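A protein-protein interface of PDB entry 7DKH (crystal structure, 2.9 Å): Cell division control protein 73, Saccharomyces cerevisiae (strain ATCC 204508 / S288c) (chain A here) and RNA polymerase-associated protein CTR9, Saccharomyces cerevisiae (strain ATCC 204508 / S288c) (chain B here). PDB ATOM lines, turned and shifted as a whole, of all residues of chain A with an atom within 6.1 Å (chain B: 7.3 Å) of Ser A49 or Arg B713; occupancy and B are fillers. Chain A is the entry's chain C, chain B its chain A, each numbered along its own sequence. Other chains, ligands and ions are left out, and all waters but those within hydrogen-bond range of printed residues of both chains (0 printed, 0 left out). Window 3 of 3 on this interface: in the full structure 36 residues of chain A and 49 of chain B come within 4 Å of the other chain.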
ATOM      1  N   LEU A  44     -16.600 -21.384 -17.234  1.00  0.00           N
ATOM      2  CA  LEU A  44     -16.213 -20.213 -16.453  1.00  0.00           C
ATOM      3  C   LEU A  44     -14.738 -19.875 -16.570  1.00  0.00           C
ATOM      4  O   LEU A  44     -14.374 -18.697 -16.485  1.00  0.00           O
ATOM      5  CB  LEU A  44     -16.505 -20.413 -14.959  1.00  0.00           C
ATOM      6  CG  LEU A  44     -17.792 -20.944 -14.341  1.00  0.00           C
ATOM      7  CD1 LEU A  44     -17.572 -21.120 -12.848  1.00  0.00           C
ATOM      8  CD2 LEU A  44     -18.909 -19.949 -14.584  1.00  0.00           C
ATOM      9  N   LYS A  45     -13.886 -20.877 -16.767  1.00  0.00           N
ATOM     10  CA  LYS A  45     -12.450 -20.666 -16.820  1.00  0.00           C
ATOM     11  C   LYS A  45     -11.891 -20.571 -18.234  1.00  0.00           C
ATOM     12  O   LYS A  45     -10.791 -20.036 -18.406  1.00  0.00           O
ATOM     13  CB  LYS A  45     -11.747 -21.795 -16.057  1.00  0.00           C
ATOM     14  CG  LYS A  45     -12.468 -22.144 -14.762  1.00  0.00           C
ATOM     15  CD  LYS A  45     -11.867 -23.349 -14.060  1.00  0.00           C
ATOM     16  CE  LYS A  45     -10.749 -22.967 -13.109  1.00  0.00           C
ATOM     17  NZ  LYS A  45     -10.595 -24.008 -12.051  1.00  0.00           N
ATOM     18  N   LEU A  46     -12.615 -21.044 -19.249  1.00  0.00           N
ATOM     19  CA  LEU A  46     -12.133 -20.953 -20.621  1.00  0.00           C
ATOM     20  C   LEU A  46     -13.002 -20.055 -21.498  1.00  0.00           C
ATOM     21  O   LEU A  46     -12.518 -19.026 -21.976  1.00  0.00           O
ATOM     22  CB  LEU A  46     -12.050 -22.360 -21.236  1.00  0.00           C
ATOM     23  CG  LEU A  46     -11.104 -23.352 -20.550  1.00  0.00           C
ATOM     24  CD1 LEU A  46     -11.251 -24.744 -21.144  1.00  0.00           C
ATOM     25  CD2 LEU A  46      -9.666 -22.879 -20.637  1.00  0.00           C
ATOM     26  N   VAL A  47     -14.292 -20.374 -21.651  1.00  0.00           N
ATOM     27  CA  VAL A  47     -15.106 -19.702 -22.667  1.00  0.00           C
ATOM     28  C   VAL A  47     -15.119 -18.200 -22.422  1.00  0.00           C
ATOM     29  O   VAL A  47     -14.780 -17.403 -23.307  1.00  0.00           O
ATOM     30  CB  VAL A  47     -16.533 -20.280 -22.684  1.00  0.00           C
ATOM     31  CG1 VAL A  47     -17.428 -19.438 -23.577  1.00  0.00           C
ATOM     32  CG2 VAL A  47     -16.525 -21.735 -23.143  1.00  0.00           C
ATOM     33  N   GLN A  48     -15.411 -17.803 -21.184  1.00  0.00           N
ATOM     34  CA  GLN A  48     -15.540 -16.389 -20.871  1.00  0.00           C
ATOM     35  C   GLN A  48     -14.195 -15.691 -20.978  1.00  0.00           C
ATOM     36  O   GLN A  48     -14.139 -14.489 -21.261  1.00  0.00           O
ATOM     37  CB  GLN A  48     -16.113 -16.230 -19.467  1.00  0.00           C
ATOM     38  CG  GLN A  48     -17.606 -16.462 -19.393  1.00  0.00           C
ATOM     39  CD  GLN A  48     -18.132 -16.355 -17.986  1.00  0.00           C
ATOM     40  OE1 GLN A  48     -17.443 -15.871 -17.087  1.00  0.00           O
ATOM     41  NE2 GLN A  48     -19.347 -16.848 -17.773  1.00  0.00           N
ATOM     42  N   SER A  49     -13.105 -16.427 -20.755  1.00  0.00           N
ATOM     43  CA  SER A  49     -11.782 -15.859 -20.956  1.00  0.00           C
ATOM     44  C   SER A  49     -11.361 -15.925 -22.418  1.00  0.00           C
ATOM     45  O   SER A  49     -10.609 -15.060 -22.878  1.00  0.00           O
ATOM     46  CB  SER A  49     -10.756 -16.594 -20.087  1.00  0.00           C
ATOM     47  OG  SER A  49     -11.136 -16.601 -18.721  1.00  0.00           O
ATOM     48  N   ILE A  50     -11.836 -16.929 -23.163  1.00  0.00           N
ATOM     49  CA  ILE A  50     -11.576 -16.960 -24.598  1.00  0.00           C
ATOM     50  C   ILE A  50     -12.437 -15.953 -25.349  1.00  0.00           C
ATOM     51  O   ILE A  50     -12.024 -15.448 -26.400  1.00  0.00           O
ATOM     52  CB  ILE A  50     -11.766 -18.387 -25.151  1.00  0.00           C
ATOM     53  CG1 ILE A  50     -10.803 -19.358 -24.467  1.00  0.00           C
ATOM     54  CG2 ILE A  50     -11.523 -18.432 -26.651  1.00  0.00           C
ATOM     55  CD1 ILE A  50      -9.360 -18.904 -24.488  1.00  0.00           C
ATOM     56  N   LYS A  51     -13.618 -15.620 -24.827  1.00  0.00           N
ATOM     57  CA  LYS A  51     -14.484 -14.686 -25.538  1.00  0.00           C
ATOM     58  C   LYS A  51     -14.052 -13.238 -25.369  1.00  0.00           C
ATOM     59  O   LYS A  51     -14.780 -12.340 -25.808  1.00  0.00           O
ATOM     60  CB  LYS A  51     -15.939 -14.858 -25.093  1.00  0.00           C
ATOM     61  CG  LYS A  51     -16.670 -15.973 -25.835  1.00  0.00           C
ATOM     62  CD  LYS A  51     -18.200 -15.870 -25.753  1.00  0.00           C
ATOM     63  CE  LYS A  51     -18.717 -15.286 -24.442  1.00  0.00           C
ATOM     64  NZ  LYS A  51     -18.180 -15.993 -23.249  1.00  0.00           N
ATOM     65  N   GLY A  52     -12.902 -12.989 -24.745  1.00  0.00           N
ATOM     66  CA  GLY A  52     -12.326 -11.661 -24.718  1.00  0.00           C
ATOM     67  C   GLY A  52     -11.638 -11.371 -26.033  1.00  0.00           C
ATOM     68  O   GLY A  52     -10.416 -11.197 -26.085  1.00  0.00           O
ATOM     69  N   SER A  53     -12.423 -11.318 -27.107  1.00  0.00           N
ATOM     70  CA  SER A  53     -11.900 -11.062 -28.441  1.00  0.00           C
ATOM     71  C   SER A  53     -12.979 -10.510 -29.362  1.00  0.00           C
ATOM     72  O   SER A  53     -12.741 -10.291 -30.550  1.00  0.00           O
ATOM     73  CB  SER A  53     -11.320 -12.345 -29.036  1.00  0.00           C
ATOM     74  OG  SER A  53     -10.408 -12.944 -28.139  1.00  0.00           O
ATOM     75  N   LYS B 677      -9.416 -18.631 -31.986  1.00  0.00           N
ATOM     76  CA  LYS B 677     -10.288 -18.396 -30.846  1.00  0.00           C
ATOM     77  C   LYS B 677     -11.636 -19.073 -31.056  1.00  0.00           C
ATOM     78  O   LYS B 677     -12.263 -19.536 -30.095  1.00  0.00           O
ATOM     79  CB  LYS B 677     -10.467 -16.893 -30.634  1.00  0.00           C
ATOM     80  CG  LYS B 677      -9.164 -16.105 -30.680  1.00  0.00           C
ATOM     81  CD  LYS B 677      -8.956 -15.268 -29.432  1.00  0.00           C
ATOM     82  CE  LYS B 677      -7.700 -14.414 -29.535  1.00  0.00           C
ATOM     83  NZ  LYS B 677      -8.020 -12.959 -29.607  1.00  0.00           N
ATOM     84  N   ALA B 705      -8.702 -30.709 -20.519  1.00  0.00           N
ATOM     85  CA  ALA B 705      -7.483 -30.422 -19.765  1.00  0.00           C
ATOM     86  C   ALA B 705      -6.371 -29.909 -20.672  1.00  0.00           C
ATOM     87  O   ALA B 705      -5.602 -29.023 -20.284  1.00  0.00           O
ATOM     88  CB  ALA B 705      -7.031 -31.672 -19.014  1.00  0.00           C
ATOM     89  N   ILE B 706      -6.255 -30.480 -21.870  1.00  0.00           N
ATOM     90  CA  ILE B 706      -5.285 -29.996 -22.849  1.00  0.00           C
ATOM     91  C   ILE B 706      -5.584 -28.549 -23.228  1.00  0.00           C
ATOM     92  O   ILE B 706      -4.673 -27.716 -23.328  1.00  0.00           O
ATOM     93  CB  ILE B 706      -5.274 -30.925 -24.076  1.00  0.00           C
ATOM     94  CG1 ILE B 706      -4.667 -32.274 -23.687  1.00  0.00           C
ATOM     95  CG2 ILE B 706      -4.513 -30.292 -25.221  1.00  0.00           C
ATOM     96  CD1 ILE B 706      -4.557 -33.263 -24.820  1.00  0.00           C
ATOM     97  N   ILE B 707      -6.864 -28.225 -23.441  1.00  0.00           N
ATOM     98  CA  ILE B 707      -7.216 -26.837 -23.744  1.00  0.00           C
ATOM     99  C   ILE B 707      -6.946 -25.940 -22.540  1.00  0.00           C
ATOM    100  O   ILE B 707      -6.582 -24.767 -22.693  1.00  0.00           O
ATOM    101  CB  ILE B 707      -8.687 -26.740 -24.204  1.00  0.00           C
ATOM    102  CG1 ILE B 707      -8.901 -27.526 -25.496  1.00  0.00           C
ATOM    103  CG2 ILE B 707      -9.110 -25.287 -24.402  1.00  0.00           C
ATOM    104  CD1 ILE B 707     -10.292 -27.368 -26.074  1.00  0.00           C
ATOM    105  N   PHE B 708      -7.101 -26.479 -21.329  1.00  0.00           N
ATOM    106  CA  PHE B 708      -6.736 -25.742 -20.124  1.00  0.00           C
ATOM    107  C   PHE B 708      -5.244 -25.439 -20.095  1.00  0.00           C
ATOM    108  O   PHE B 708      -4.829 -24.351 -19.682  1.00  0.00           O
ATOM    109  CB  PHE B 708      -7.129 -26.546 -18.885  1.00  0.00           C
ATOM    110  CG  PHE B 708      -8.438 -26.144 -18.278  1.00  0.00           C
ATOM    111  CD1 PHE B 708      -8.553 -24.957 -17.574  1.00  0.00           C
ATOM    112  CD2 PHE B 708      -9.551 -26.958 -18.398  1.00  0.00           C
ATOM    113  CE1 PHE B 708      -9.754 -24.589 -17.007  1.00  0.00           C
ATOM    114  CE2 PHE B 708     -10.756 -26.594 -17.836  1.00  0.00           C
ATOM    115  CZ  PHE B 708     -10.858 -25.409 -17.139  1.00  0.00           C
ATOM    116  N   ALA B 709      -4.422 -26.398 -20.521  1.00  0.00           N
ATOM    117  CA  ALA B 709      -2.977 -26.220 -20.454  1.00  0.00           C
ATOM    118  C   ALA B 709      -2.476 -25.296 -21.551  1.00  0.00           C
ATOM    119  O   ALA B 709      -1.476 -24.598 -21.355  1.00  0.00           O
ATOM    120  CB  ALA B 709      -2.268 -27.573 -20.540  1.00  0.00           C
ATOM    121  N   GLU B 710      -3.148 -25.280 -22.704  1.00  0.00           N
ATOM    122  CA  GLU B 710      -2.763 -24.398 -23.799  1.00  0.00           C
ATOM    123  C   GLU B 710      -3.310 -22.983 -23.642  1.00  0.00           C
ATOM    124  O   GLU B 710      -2.950 -22.107 -24.436  1.00  0.00           O
ATOM    125  CB  GLU B 710      -3.210 -25.009 -25.130  1.00  0.00           C
ATOM    126  CG  GLU B 710      -2.663 -26.420 -25.331  1.00  0.00           C
ATOM    127  CD  GLU B 710      -2.828 -26.933 -26.747  1.00  0.00           C
ATOM    128  OE1 GLU B 710      -3.552 -26.292 -27.537  1.00  0.00           O
ATOM    129  OE2 GLU B 710      -2.226 -27.980 -27.073  1.00  0.00           O
ATOM    130  N   SER B 711      -4.167 -22.740 -22.648  1.00  0.00           N
ATOM    131  CA  SER B 711      -4.423 -21.398 -22.143  1.00  0.00           C
ATOM    132  C   SER B 711      -3.516 -21.046 -20.967  1.00  0.00           C
ATOM    133  O   SER B 711      -3.790 -20.074 -20.252  1.00  0.00           O
ATOM    134  CB  SER B 711      -5.891 -21.247 -21.736  1.00  0.00           C
ATOM    135  OG  SER B 711      -6.753 -21.923 -22.634  1.00  0.00           O
ATOM    136  N   LYS B 712      -2.447 -21.816 -20.767  1.00  0.00           N
ATOM    137  CA  LYS B 712      -1.544 -21.696 -19.618  1.00  0.00           C
ATOM    138  C   LYS B 712      -2.296 -21.610 -18.289  1.00  0.00           C
ATOM    139  O   LYS B 712      -1.964 -20.822 -17.400  1.00  0.00           O
ATOM    140  CB  LYS B 712      -0.601 -20.511 -19.791  1.00  0.00           C
ATOM    141  CG  LYS B 712       0.299 -20.643 -20.999  1.00  0.00           C
ATOM    142  CD  LYS B 712       1.269 -21.798 -20.806  1.00  0.00           C
ATOM    143  CE  LYS B 712       2.095 -22.042 -22.052  1.00  0.00           C
ATOM    144  NZ  LYS B 712       3.388 -22.700 -21.728  1.00  0.00           N
ATOM    145  N   ARG B 713      -3.331 -22.435 -18.164  1.00  0.00           N
ATOM    146  CA  ARG B 713      -3.981 -22.729 -16.887  1.00  0.00           C
ATOM    147  C   ARG B 713      -3.530 -24.127 -16.463  1.00  0.00           C
ATOM    148  O   ARG B 713      -4.218 -25.119 -16.699  1.00  0.00           O
ATOM    149  CB  ARG B 713      -5.500 -22.615 -17.024  1.00  0.00           C
ATOM    150  CG  ARG B 713      -5.936 -21.368 -17.779  1.00  0.00           C
ATOM    151  CD  ARG B 713      -7.340 -20.922 -17.398  1.00  0.00           C
ATOM    152  NE  ARG B 713      -7.383 -20.277 -16.089  1.00  0.00           N
ATOM    153  CZ  ARG B 713      -8.370 -19.489 -15.677  1.00  0.00           C
ATOM    154  NH1 ARG B 713      -9.395 -19.234 -16.479  1.00  0.00           N
ATOM    155  NH2 ARG B 713      -8.330 -18.948 -14.468  1.00  0.00           N
ATOM    156  N   LEU B 714      -2.348 -24.202 -15.839  1.00  0.00           N
ATOM    157  CA  LEU B 714      -1.707 -25.494 -15.601  1.00  0.00           C
ATOM    158  C   LEU B 714      -2.192 -26.210 -14.345  1.00  0.00           C
ATOM    159  O   LEU B 714      -2.083 -27.440 -14.276  1.00  0.00           O
ATOM    160  CB  LEU B 714      -0.186 -25.319 -15.528  1.00  0.00           C
ATOM    161  CG  LEU B 714       0.508 -24.782 -16.787  1.00  0.00           C
ATOM    162  CD1 LEU B 714       2.011 -24.738 -16.599  1.00  0.00           C
ATOM    163  CD2 LEU B 714       0.157 -25.617 -18.008  1.00  0.00           C
ATOM    164  N   GLY B 715      -2.717 -25.486 -13.360  1.00  0.00           N
ATOM    165  CA  GLY B 715      -3.282 -26.089 -12.172  1.00  0.00           C
ATOM    166  C   GLY B 715      -4.460 -26.998 -12.470  1.00  0.00           C
ATOM    167  O   GLY B 715      -4.463 -28.197 -12.145  1.00  0.00           O
ATOM    168  N   PRO B 716      -5.514 -26.420 -13.060  1.00  0.00           N
ATOM    169  CA  PRO B 716      -6.665 -27.249 -13.456  1.00  0.00           C
ATOM    170  C   PRO B 716      -6.287 -28.357 -14.420  1.00  0.00           C
ATOM    171  O   PRO B 716      -6.799 -29.480 -14.306  1.00  0.00           O
ATOM    172  CB  PRO B 716      -7.622 -26.232 -14.096  1.00  0.00           C
ATOM    173  CG  PRO B 716      -7.228 -24.911 -13.502  1.00  0.00           C
ATOM    174  CD  PRO B 716      -5.752 -24.984 -13.295  1.00  0.00           C
ATOM    175  N   ALA B 717      -5.407 -28.064 -15.382  1.00  0.00           N
ATOM    176  CA  ALA B 717      -4.984 -29.090 -16.327  1.00  0.00           C
ATOM    177  C   ALA B 717      -4.323 -30.255 -15.606  1.00  0.00           C
ATOM    178  O   ALA B 717      -4.616 -31.420 -15.898  1.00  0.00           O
ATOM    179  CB  ALA B 717      -4.034 -28.490 -17.363  1.00  0.00           C
ATOM    180  N   LEU B 718      -3.456 -29.962 -14.633  1.00  0.00           N
ATOM    181  CA  LEU B 718      -2.780 -31.037 -13.921  1.00  0.00           C
ATOM    182  C   LEU B 718      -3.757 -31.832 -13.067  1.00  0.00           C
ATOM    183  O   LEU B 718      -3.629 -33.055 -12.955  1.00  0.00           O
ATOM    184  CB  LEU B 718      -1.641 -30.487 -13.063  1.00  0.00           C
ATOM    185  CG  LEU B 718      -0.813 -31.592 -12.399  1.00  0.00           C
ATOM    186  CD1 LEU B 718       0.030 -32.324 -13.436  1.00  0.00           C
ATOM    187  CD2 LEU B 718       0.069 -31.044 -11.293  1.00  0.00           C
ATOM    188  N   ILE B 720      -6.961 -32.350 -13.677  1.00  0.00           N
ATOM    189  CA  ILE B 720      -7.747 -33.202 -14.566  1.00  0.00           C
ATOM    190  C   ILE B 720      -6.898 -34.363 -15.069  1.00  0.00           C
ATOM    191  O   ILE B 720      -7.380 -35.495 -15.177  1.00  0.00           O
ATOM    192  CB  ILE B 720      -8.338 -32.402 -15.746  1.00  0.00           C
ATOM    193  CG1 ILE B 720      -9.218 -31.243 -15.276  1.00  0.00           C
ATOM    194  CG2 ILE B 720      -9.138 -33.329 -16.658  1.00  0.00           C
ATOM    195  CD1 ILE B 720      -9.387 -30.163 -16.341  1.00  0.00           C
ATOM    196  N   CYS B 740       3.071 -31.327 -18.791  1.00  0.00           N
ATOM    197  CA  CYS B 740       2.494 -30.274 -17.974  1.00  0.00           C
ATOM    198  C   CYS B 740       3.412 -29.944 -16.812  1.00  0.00           C
ATOM    199  O   CYS B 740       3.561 -28.774 -16.456  1.00  0.00           O
ATOM    200  CB  CYS B 740       1.105 -30.695 -17.482  1.00  0.00           C
ATOM    201  SG  CYS B 740       0.341 -29.589 -16.269  1.00  0.00           S
ATOM    202  N   GLU B 743       6.079 -27.580 -18.145  1.00  0.00           N
ATOM    203  CA  GLU B 743       5.607 -26.210 -18.285  1.00  0.00           C
ATOM    204  C   GLU B 743       5.397 -25.512 -16.941  1.00  0.00           C
ATOM    205  O   GLU B 743       5.251 -24.286 -16.925  1.00  0.00           O
ATOM    206  CB  GLU B 743       4.315 -26.197 -19.105  1.00  0.00           C
ATOM    207  CG  GLU B 743       4.476 -26.656 -20.558  1.00  0.00           C
ATOM    208  CD  GLU B 743       3.487 -25.987 -21.503  1.00  0.00           C
ATOM    209  OE1 GLU B 743       2.346 -25.705 -21.076  1.00  0.00           O
ATOM    210  OE2 GLU B 743       3.848 -25.753 -22.675  1.00  0.00           O
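The side-chain hydroxyl (OG) of Ser A53 lies within hydrogen-bond range of the side-chain amino group (NZ) of Lys B677 (2.8 Å). O of Lys A45 sits at hydrogen-bond distance from NH1 of Arg B713 (2.5 Å).
The backbone carbonyl oxygen (O) of Ile B707 sits at hydrogen-bond distance from the side-chain hydroxyl (OG) of Ser B711 (2.8 Å). O of Phe B708 lies within hydrogen-bond range of N of Arg B713. The backbone carbonyl oxygen (O) of Lys A45 sits at hydrogen-bond distance from the side-chain hydroxyl (OG) of Ser A49 (3.5 Å). The backbone carbonyl oxygen (O) of Ile A50 is in hydrogen-bond range of the side-chain hydroxyl (OG) of Ser A53 (3.5 Å).
Lys A45 touches Phe B708 (CB to CE1, 3.6 Å). Lys A45 touches Pro B716 (NZ to CG, 3.8 Å). CD1 of Leu A46 touches CG2 of Ile B707 (3.9 Å). Leu A46 touches Phe B708 (CD1 to CE2, 3.8 Å). Ser B711 touches Leu A46. Ser A49 touches Arg B713 (OG to NH1, 3.9 Å). Lys B677 touches Ile A50 (O to CG2, 3.7 Å).
Ser A49 touches just one residue of chain B: Arg B713 (3.9 Å). Of the printed residues of chain B, Ser A53 touches Lys B677 (2.8 Å). Of the printed residues of chain A, Ile B707 touches Leu A46. Of the printed residues of chain A, Phe B708 touches Lys A45 and Leu A46. Arg B713 touches just these residues of chain A: Lys A45 (2.5 Å) and Ser A49 (3.9 Å). Glu B743 touches none of the printed residues of chain A. The nearest printed residue of chain B that does not touch Ser A53 is Ser B711 (11.1 Å).
Of the 10 printed residues of chain A, 5 touch a printed residue of chain B. Hydrophobic or aromatic side chains of chain A that line the printed part of chain B: Leu A46 and Ile A50. Hydrophobic or aromatic side chains of chain B that line the printed part of chain A: Ile B707, Phe B708 and Pro B716.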
